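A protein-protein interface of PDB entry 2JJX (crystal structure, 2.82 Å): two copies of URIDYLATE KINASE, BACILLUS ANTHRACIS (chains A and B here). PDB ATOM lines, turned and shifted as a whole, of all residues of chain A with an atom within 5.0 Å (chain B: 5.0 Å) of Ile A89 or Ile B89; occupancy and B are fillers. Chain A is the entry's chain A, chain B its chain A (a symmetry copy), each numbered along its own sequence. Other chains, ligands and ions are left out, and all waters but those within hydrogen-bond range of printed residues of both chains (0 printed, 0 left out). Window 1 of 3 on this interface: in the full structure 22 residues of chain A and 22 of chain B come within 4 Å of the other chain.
Among the printed residues, merely in contact across the chains: Ile A82 with Ile B89 (3.9 Å), Ile A82 with Leu B92 (3.5 Å), Ile A82 with Met B93 (3.9 Å), Leu A85 with Ile B88 (3.7 Å), Leu A85 with Ile B89 (3.5 Å), Leu A85 with Leu B92 (3.7 Å), Ile A88 with Leu B85 (3.7 Å), Ile A89 with Ile B82 (3.9 Å), Ile A89 with Leu B85 (3.5 Å), Ile A89 with Ile B89 (3.2 Å), Leu A92 with Ile B82 (3.5 Å), Leu A92 with Leu B85 (3.7 Å) and Met A93 with Ile B82 (3.9 Å).
Ile A89 touches just these residues of chain B: Ile B82, Leu B85 and Ile B89. Ile B89 touches three residues of chain A. Printed residues of chain B within 4 Å of Leu A85: Ile B88 (3.7 Å), Ile B89 (3.5 Å) and Leu B92 (3.7 Å). Printed residues of chain A within 4 Å of Leu B85: Ile A88, Ile A89 and Leu A92. Of the printed residues of chain A, Leu B92 touches Ile A82 (3.5 Å) and Leu A85 (3.7 Å). Asn B90 touches none of the printed residues of chain A. Phe B32 touches none of the printed residues of chain A. The nearest printed residue of chain A that does not touch Ile B88 is Ile A82 (6.0 Å).
Of the 12 printed residues of chain A, 6 touch a printed residue of chain B. Hydrophobic or aromatic side chains of chain A that line the printed part of chain B: Ile A82, Leu A85, Ile A88, Ile A89 and Leu A92. Of the 12 printed residues of chain B, 6 touch a printed residue of chain A. Hydrophobic or aromatic side chains of chain B within 4 Å of the printed part of chain A: Ile B82, Leu B85, Ile B88, Ile B89 and Leu B92. Among the printed residues, no Asp or Glu carboxylate lies within 4 Å of a Lys or Arg side-chain nitrogen of the other chain.
Ile A82 touches Leu B92, and with the chains exchanged Leu A92 touches Ile B82. Ile A82 touches Met B93, and with the chains exchanged Met A93 touches Ile B82. Leu A85 touches Ile B89, and with the chains exchanged Ile A89 touches Leu B85. Ile B89 touches its own counterpart, Ile A89. Of the 13 pairs that touch across the chains among the printed residues, 13 have their exchanged pair printed and touching as well.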
ATOM      1  N   PHE A  32       5.040  22.235 -22.337  1.00  0.00           N
ATOM      2  CA  PHE A  32       5.017  20.913 -22.928  1.00  0.00           C
ATOM      3  C   PHE A  32       3.661  20.630 -23.516  1.00  0.00           C
ATOM      4  O   PHE A  32       2.651  21.125 -23.044  1.00  0.00           O
ATOM      5  CB  PHE A  32       5.346  19.850 -21.896  1.00  0.00           C
ATOM      6  CG  PHE A  32       6.638  20.093 -21.186  1.00  0.00           C
ATOM      7  CD1 PHE A  32       6.684  20.975 -20.123  1.00  0.00           C
ATOM      8  CD2 PHE A  32       7.806  19.460 -21.587  1.00  0.00           C
ATOM      9  CE1 PHE A  32       7.851  21.193 -19.453  1.00  0.00           C
ATOM     10  CE2 PHE A  32       8.970  19.668 -20.906  1.00  0.00           C
ATOM     11  CZ  PHE A  32       8.996  20.548 -19.846  1.00  0.00           C
ATOM     12  N   ILE A  63      10.926  26.862 -22.642  1.00  0.00           N
ATOM     13  CA  ILE A  63      10.831  27.395 -21.290  1.00  0.00           C
ATOM     14  C   ILE A  63      11.352  28.820 -21.225  1.00  0.00           C
ATOM     15  O   ILE A  63      10.731  29.690 -20.632  1.00  0.00           O
ATOM     16  CB  ILE A  63      11.639  26.525 -20.312  1.00  0.00           C
ATOM     17  CG1 ILE A  63      11.131  25.091 -20.291  1.00  0.00           C
ATOM     18  CG2 ILE A  63      11.708  27.168 -18.948  1.00  0.00           C
ATOM     19  CD1 ILE A  63      11.986  24.219 -19.409  1.00  0.00           C
ATOM     20  N   ILE A  82      20.307  30.302 -17.238  1.00  0.00           N
ATOM     21  CA  ILE A  82      18.885  30.069 -17.036  1.00  0.00           C
ATOM     22  C   ILE A  82      18.404  29.119 -18.101  1.00  0.00           C
ATOM     23  O   ILE A  82      17.762  28.111 -17.809  1.00  0.00           O
ATOM     24  CB  ILE A  82      18.089  31.380 -17.057  1.00  0.00           C
ATOM     25  CG1 ILE A  82      18.558  32.309 -15.929  1.00  0.00           C
ATOM     26  CG2 ILE A  82      16.591  31.114 -16.969  1.00  0.00           C
ATOM     27  CD1 ILE A  82      17.947  33.698 -15.961  1.00  0.00           C
ATOM     28  N   LEU A  85      19.146  25.506 -17.475  1.00  0.00           N
ATOM     29  CA  LEU A  85      18.327  24.805 -16.488  1.00  0.00           C
ATOM     30  C   LEU A  85      17.114  24.257 -17.235  1.00  0.00           C
ATOM     31  O   LEU A  85      16.578  23.204 -16.870  1.00  0.00           O
ATOM     32  CB  LEU A  85      17.878  25.757 -15.373  1.00  0.00           C
ATOM     33  CG  LEU A  85      18.589  25.693 -14.022  1.00  0.00           C
ATOM     34  CD1 LEU A  85      19.934  25.007 -14.177  1.00  0.00           C
ATOM     35  CD2 LEU A  85      18.773  27.100 -13.474  1.00  0.00           C
ATOM     36  N   GLY A  86      16.717  24.958 -18.303  1.00  0.00           N
ATOM     37  CA  GLY A  86      15.612  24.555 -19.159  1.00  0.00           C
ATOM     38  C   GLY A  86      15.845  23.192 -19.795  1.00  0.00           C
ATOM     39  O   GLY A  86      14.948  22.363 -19.858  1.00  0.00           O
ATOM     40  N   THR A  87      17.056  22.980 -20.304  1.00  0.00           N
ATOM     41  CA  THR A  87      17.429  21.735 -20.969  1.00  0.00           C
ATOM     42  C   THR A  87      17.334  20.572 -20.007  1.00  0.00           C
ATOM     43  O   THR A  87      17.014  19.467 -20.429  1.00  0.00           O
ATOM     44  CB  THR A  87      18.826  21.782 -21.629  1.00  0.00           C
ATOM     45  OG1 THR A  87      19.860  21.721 -20.635  1.00  0.00           O
ATOM     46  CG2 THR A  87      19.004  23.053 -22.474  1.00  0.00           C
ATOM     47  N   ILE A  88      17.662  20.800 -18.730  1.00  0.00           N
ATOM     48  CA  ILE A  88      17.646  19.737 -17.712  1.00  0.00           C
ATOM     49  C   ILE A  88      16.220  19.330 -17.364  1.00  0.00           C
ATOM     50  O   ILE A  88      15.908  18.144 -17.162  1.00  0.00           O
ATOM     51  CB  ILE A  88      18.463  20.106 -16.485  1.00  0.00           C
ATOM     52  CG1 ILE A  88      19.937  20.204 -16.863  1.00  0.00           C
ATOM     53  CG2 ILE A  88      18.361  19.047 -15.413  1.00  0.00           C
ATOM     54  CD1 ILE A  88      20.662  21.271 -16.156  1.00  0.00           C
ATOM     55  N   ILE A  89      15.354  20.338 -17.324  1.00  0.00           N
ATOM     56  CA  ILE A  89      13.936  20.135 -17.053  1.00  0.00           C
ATOM     57  C   ILE A  89      13.356  19.272 -18.167  1.00  0.00           C
ATOM     58  O   ILE A  89      12.682  18.289 -17.904  1.00  0.00           O
ATOM     59  CB  ILE A  89      13.196  21.486 -16.934  1.00  0.00           C
ATOM     60  CG1 ILE A  89      13.626  22.228 -15.673  1.00  0.00           C
ATOM     61  CG2 ILE A  89      11.697  21.322 -17.013  1.00  0.00           C
ATOM     62  CD1 ILE A  89      12.936  23.568 -15.520  1.00  0.00           C
ATOM     63  N   ASN A  90      13.662  19.626 -19.412  1.00  0.00           N
ATOM     64  CA  ASN A  90      13.179  18.892 -20.579  1.00  0.00           C
ATOM     65  C   ASN A  90      13.742  17.475 -20.599  1.00  0.00           C
ATOM     66  O   ASN A  90      13.049  16.536 -20.989  1.00  0.00           O
ATOM     67  CB  ASN A  90      13.584  19.594 -21.871  1.00  0.00           C
ATOM     68  CG  ASN A  90      12.751  20.833 -22.164  1.00  0.00           C
ATOM     69  OD1 ASN A  90      11.806  21.153 -21.447  1.00  0.00           O
ATOM     70  ND2 ASN A  90      13.114  21.547 -23.230  1.00  0.00           N
ATOM     71  N   SER A  91      15.007  17.329 -20.214  1.00  0.00           N
ATOM     72  CA  SER A  91      15.638  16.014 -20.175  1.00  0.00           C
ATOM     73  C   SER A  91      14.844  15.107 -19.233  1.00  0.00           C
ATOM     74  O   SER A  91      14.451  13.985 -19.579  1.00  0.00           O
ATOM     75  CB  SER A  91      17.086  16.133 -19.684  1.00  0.00           C
ATOM     76  OG  SER A  91      17.882  16.825 -20.641  1.00  0.00           O
ATOM     77  N   LEU A  92      14.598  15.627 -18.036  1.00  0.00           N
ATOM     78  CA  LEU A  92      13.872  14.890 -17.015  1.00  0.00           C
ATOM     79  C   LEU A  92      12.469  14.521 -17.466  1.00  0.00           C
ATOM     80  O   LEU A  92      12.082  13.358 -17.332  1.00  0.00           O
ATOM     81  CB  LEU A  92      13.789  15.699 -15.743  1.00  0.00           C
ATOM     82  CG  LEU A  92      14.900  15.488 -14.731  1.00  0.00           C
ATOM     83  CD1 LEU A  92      16.146  14.859 -15.335  1.00  0.00           C
ATOM     84  CD2 LEU A  92      15.166  16.829 -14.058  1.00  0.00           C
ATOM     85  N   MET A  93      11.717  15.486 -18.007  1.00  0.00           N
ATOM     86  CA  MET A  93      10.419  15.186 -18.617  1.00  0.00           C
ATOM     87  C   MET A  93      10.563  14.057 -19.628  1.00  0.00           C
ATOM     88  O   MET A  93      10.124  12.949 -19.374  1.00  0.00           O
ATOM     89  CB  MET A  93       9.838  16.397 -19.323  1.00  0.00           C
ATOM     90  CG  MET A  93       8.832  17.156 -18.472  1.00  0.00           C
ATOM     91  SD  MET A  93       7.270  16.282 -18.102  1.00  0.00           S
ATOM     92  CE  MET A  93       6.816  15.821 -19.703  1.00  0.00           C
ATOM     93  N   PHE B  32       6.583  33.331 -18.489  1.00  0.00           N
ATOM     94  CA  PHE B  32       6.709  34.617 -17.834  1.00  0.00           C
ATOM     95  C   PHE B  32       5.927  35.661 -18.585  1.00  0.00           C
ATOM     96  O   PHE B  32       5.764  35.584 -19.791  1.00  0.00           O
ATOM     97  CB  PHE B  32       8.162  35.045 -17.749  1.00  0.00           C
ATOM     98  CG  PHE B  32       9.042  34.028 -17.099  1.00  0.00           C
ATOM     99  CD1 PHE B  32       9.520  32.960 -17.834  1.00  0.00           C
ATOM    100  CD2 PHE B  32       9.379  34.126 -15.756  1.00  0.00           C
ATOM    101  CE1 PHE B  32      10.339  32.034 -17.260  1.00  0.00           C
ATOM    102  CE2 PHE B  32      10.211  33.206 -15.187  1.00  0.00           C
ATOM    103  CZ  PHE B  32      10.680  32.150 -15.936  1.00  0.00           C
ATOM    104  N   ILE B  63       6.025  26.806 -14.848  1.00  0.00           N
ATOM    105  CA  ILE B  63       6.860  26.010 -15.737  1.00  0.00           C
ATOM    106  C   ILE B  63       6.410  24.560 -15.757  1.00  0.00           C
ATOM    107  O   ILE B  63       6.294  23.952 -16.811  1.00  0.00           O
ATOM    108  CB  ILE B  63       8.330  26.069 -15.288  1.00  0.00           C
ATOM    109  CG1 ILE B  63       8.859  27.495 -15.295  1.00  0.00           C
ATOM    110  CG2 ILE B  63       9.175  25.100 -16.079  1.00  0.00           C
ATOM    111  CD1 ILE B  63      10.266  27.561 -14.761  1.00  0.00           C
ATOM    112  N   ILE B  82      11.837  17.955 -10.737  1.00  0.00           N
ATOM    113  CA  ILE B  82      11.663  18.756 -11.938  1.00  0.00           C
ATOM    114  C   ILE B  82      11.079  20.085 -11.541  1.00  0.00           C
ATOM    115  O   ILE B  82      11.589  21.140 -11.915  1.00  0.00           O
ATOM    116  CB  ILE B  82      10.779  18.043 -12.970  1.00  0.00           C
ATOM    117  CG1 ILE B  82      11.421  16.718 -13.401  1.00  0.00           C
ATOM    118  CG2 ILE B  82      10.502  18.942 -14.169  1.00  0.00           C
ATOM    119  CD1 ILE B  82      10.550  15.857 -14.297  1.00  0.00           C
ATOM    120  N   LEU B  85      13.524  22.563 -10.171  1.00  0.00           N
ATOM    121  CA  LEU B  85      14.407  23.241 -11.118  1.00  0.00           C
ATOM    122  C   LEU B  85      13.664  24.486 -11.596  1.00  0.00           C
ATOM    123  O   LEU B  85      14.289  25.507 -11.905  1.00  0.00           O
ATOM    124  CB  LEU B  85      14.738  22.331 -12.307  1.00  0.00           C
ATOM    125  CG  LEU B  85      16.106  21.655 -12.355  1.00  0.00           C
ATOM    126  CD1 LEU B  85      16.726  21.640 -10.970  1.00  0.00           C
ATOM    127  CD2 LEU B  85      15.957  20.235 -12.882  1.00  0.00           C
ATOM    128  N   GLY B  86      12.329  24.402 -11.612  1.00  0.00           N
ATOM    129  CA  GLY B  86      11.463  25.508 -11.991  1.00  0.00           C
ATOM    130  C   GLY B  86      11.651  26.720 -11.091  1.00  0.00           C
ATOM    131  O   GLY B  86      11.703  27.850 -11.556  1.00  0.00           O
ATOM    132  N   THR B  87      11.714  26.478  -9.784  1.00  0.00           N
ATOM    133  CA  THR B  87      11.867  27.536  -8.789  1.00  0.00           C
ATOM    134  C   THR B  87      13.176  28.267  -8.991  1.00  0.00           C
ATOM    135  O   THR B  87      13.246  29.461  -8.726  1.00  0.00           O
ATOM    136  CB  THR B  87      11.744  27.035  -7.332  1.00  0.00           C
ATOM    137  OG1 THR B  87      12.919  26.309  -6.942  1.00  0.00           O
ATOM    138  CG2 THR B  87      10.508  26.141  -7.149  1.00  0.00           C
ATOM    139  N   ILE B  88      14.226  27.548  -9.406  1.00  0.00           N
ATOM    140  CA  ILE B  88      15.559  28.141  -9.599  1.00  0.00           C
ATOM    141  C   ILE B  88      15.585  29.047 -10.823  1.00  0.00           C
ATOM    142  O   ILE B  88      16.209  30.122 -10.830  1.00  0.00           O
ATOM    143  CB  ILE B  88      16.656  27.091  -9.627  1.00  0.00           C
ATOM    144  CG1 ILE B  88      16.765  26.429  -8.257  1.00  0.00           C
ATOM    145  CG2 ILE B  88      18.004  27.706  -9.919  1.00  0.00           C
ATOM    146  CD1 ILE B  88      17.077  24.992  -8.315  1.00  0.00           C
ATOM    147  N   ILE B  89      14.872  28.602 -11.852  1.00  0.00           N
ATOM    148  CA  ILE B  89      14.741  29.356 -13.093  1.00  0.00           C
ATOM    149  C   ILE B  89      14.044  30.675 -12.779  1.00  0.00           C
ATOM    150  O   ILE B  89      14.508  31.732 -13.173  1.00  0.00           O
ATOM    151  CB  ILE B  89      13.971  28.543 -14.158  1.00  0.00           C
ATOM    152  CG1 ILE B  89      14.799  27.353 -14.631  1.00  0.00           C
ATOM    153  CG2 ILE B  89      13.509  29.406 -15.308  1.00  0.00           C
ATOM    154  CD1 ILE B  89      14.079  26.516 -15.668  1.00  0.00           C
ATOM    155  N   ASN B  90      12.947  30.602 -12.029  1.00  0.00           N
ATOM    156  CA  ASN B  90      12.177  31.783 -11.647  1.00  0.00           C
ATOM    157  C   ASN B  90      13.003  32.705 -10.757  1.00  0.00           C
ATOM    158  O   ASN B  90      12.903  33.926 -10.864  1.00  0.00           O
ATOM    159  CB  ASN B  90      10.911  31.388 -10.894  1.00  0.00           C
ATOM    160  CG  ASN B  90       9.824  30.832 -11.803  1.00  0.00           C
ATOM    161  OD1 ASN B  90       9.966  30.798 -13.023  1.00  0.00           O
ATOM    162  ND2 ASN B  90       8.726  30.380 -11.198  1.00  0.00           N
ATOM    163  N   SER B  91      13.790  32.120  -9.858  1.00  0.00           N
ATOM    164  CA  SER B  91      14.639  32.907  -8.970  1.00  0.00           C
ATOM    165  C   SER B  91      15.589  33.759  -9.813  1.00  0.00           C
ATOM    166  O   SER B  91      15.706  34.979  -9.641  1.00  0.00           O
ATOM    167  CB  SER B  91      15.446  31.985  -8.048  1.00  0.00           C
ATOM    168  OG  SER B  91      14.584  31.316  -7.133  1.00  0.00           O
ATOM    169  N   LEU B  92      16.255  33.090 -10.748  1.00  0.00           N
ATOM    170  CA  LEU B  92      17.212  33.744 -11.624  1.00  0.00           C
ATOM    171  C   LEU B  92      16.569  34.841 -12.455  1.00  0.00           C
ATOM    172  O   LEU B  92      17.102  35.952 -12.496  1.00  0.00           O
ATOM    173  CB  LEU B  92      17.855  32.735 -12.545  1.00  0.00           C
ATOM    174  CG  LEU B  92      19.141  32.093 -12.056  1.00  0.00           C
ATOM    175  CD1 LEU B  92      19.332  32.211 -10.553  1.00  0.00           C
ATOM    176  CD2 LEU B  92      19.150  30.654 -12.556  1.00  0.00           C
ATOM    177  N   MET B  93      15.433  34.550 -13.096  1.00  0.00           N
ATOM    178  CA  MET B  93      14.659  35.587 -13.783  1.00  0.00           C
ATOM    179  C   MET B  93      14.401  36.758 -12.844  1.00  0.00           C
ATOM    180  O   MET B  93      14.990  37.811 -13.003  1.00  0.00           O
ATOM    181  CB  MET B  93      13.325  35.059 -14.276  1.00  0.00           C
ATOM    182  CG  MET B  93      13.352  34.648 -15.741  1.00  0.00           C
ATOM    183  SD  MET B  93      13.573  36.000 -16.950  1.00  0.00           S
ATOM    184  CE  MET B  93      12.325  37.068 -16.415  1.00  0.00           C
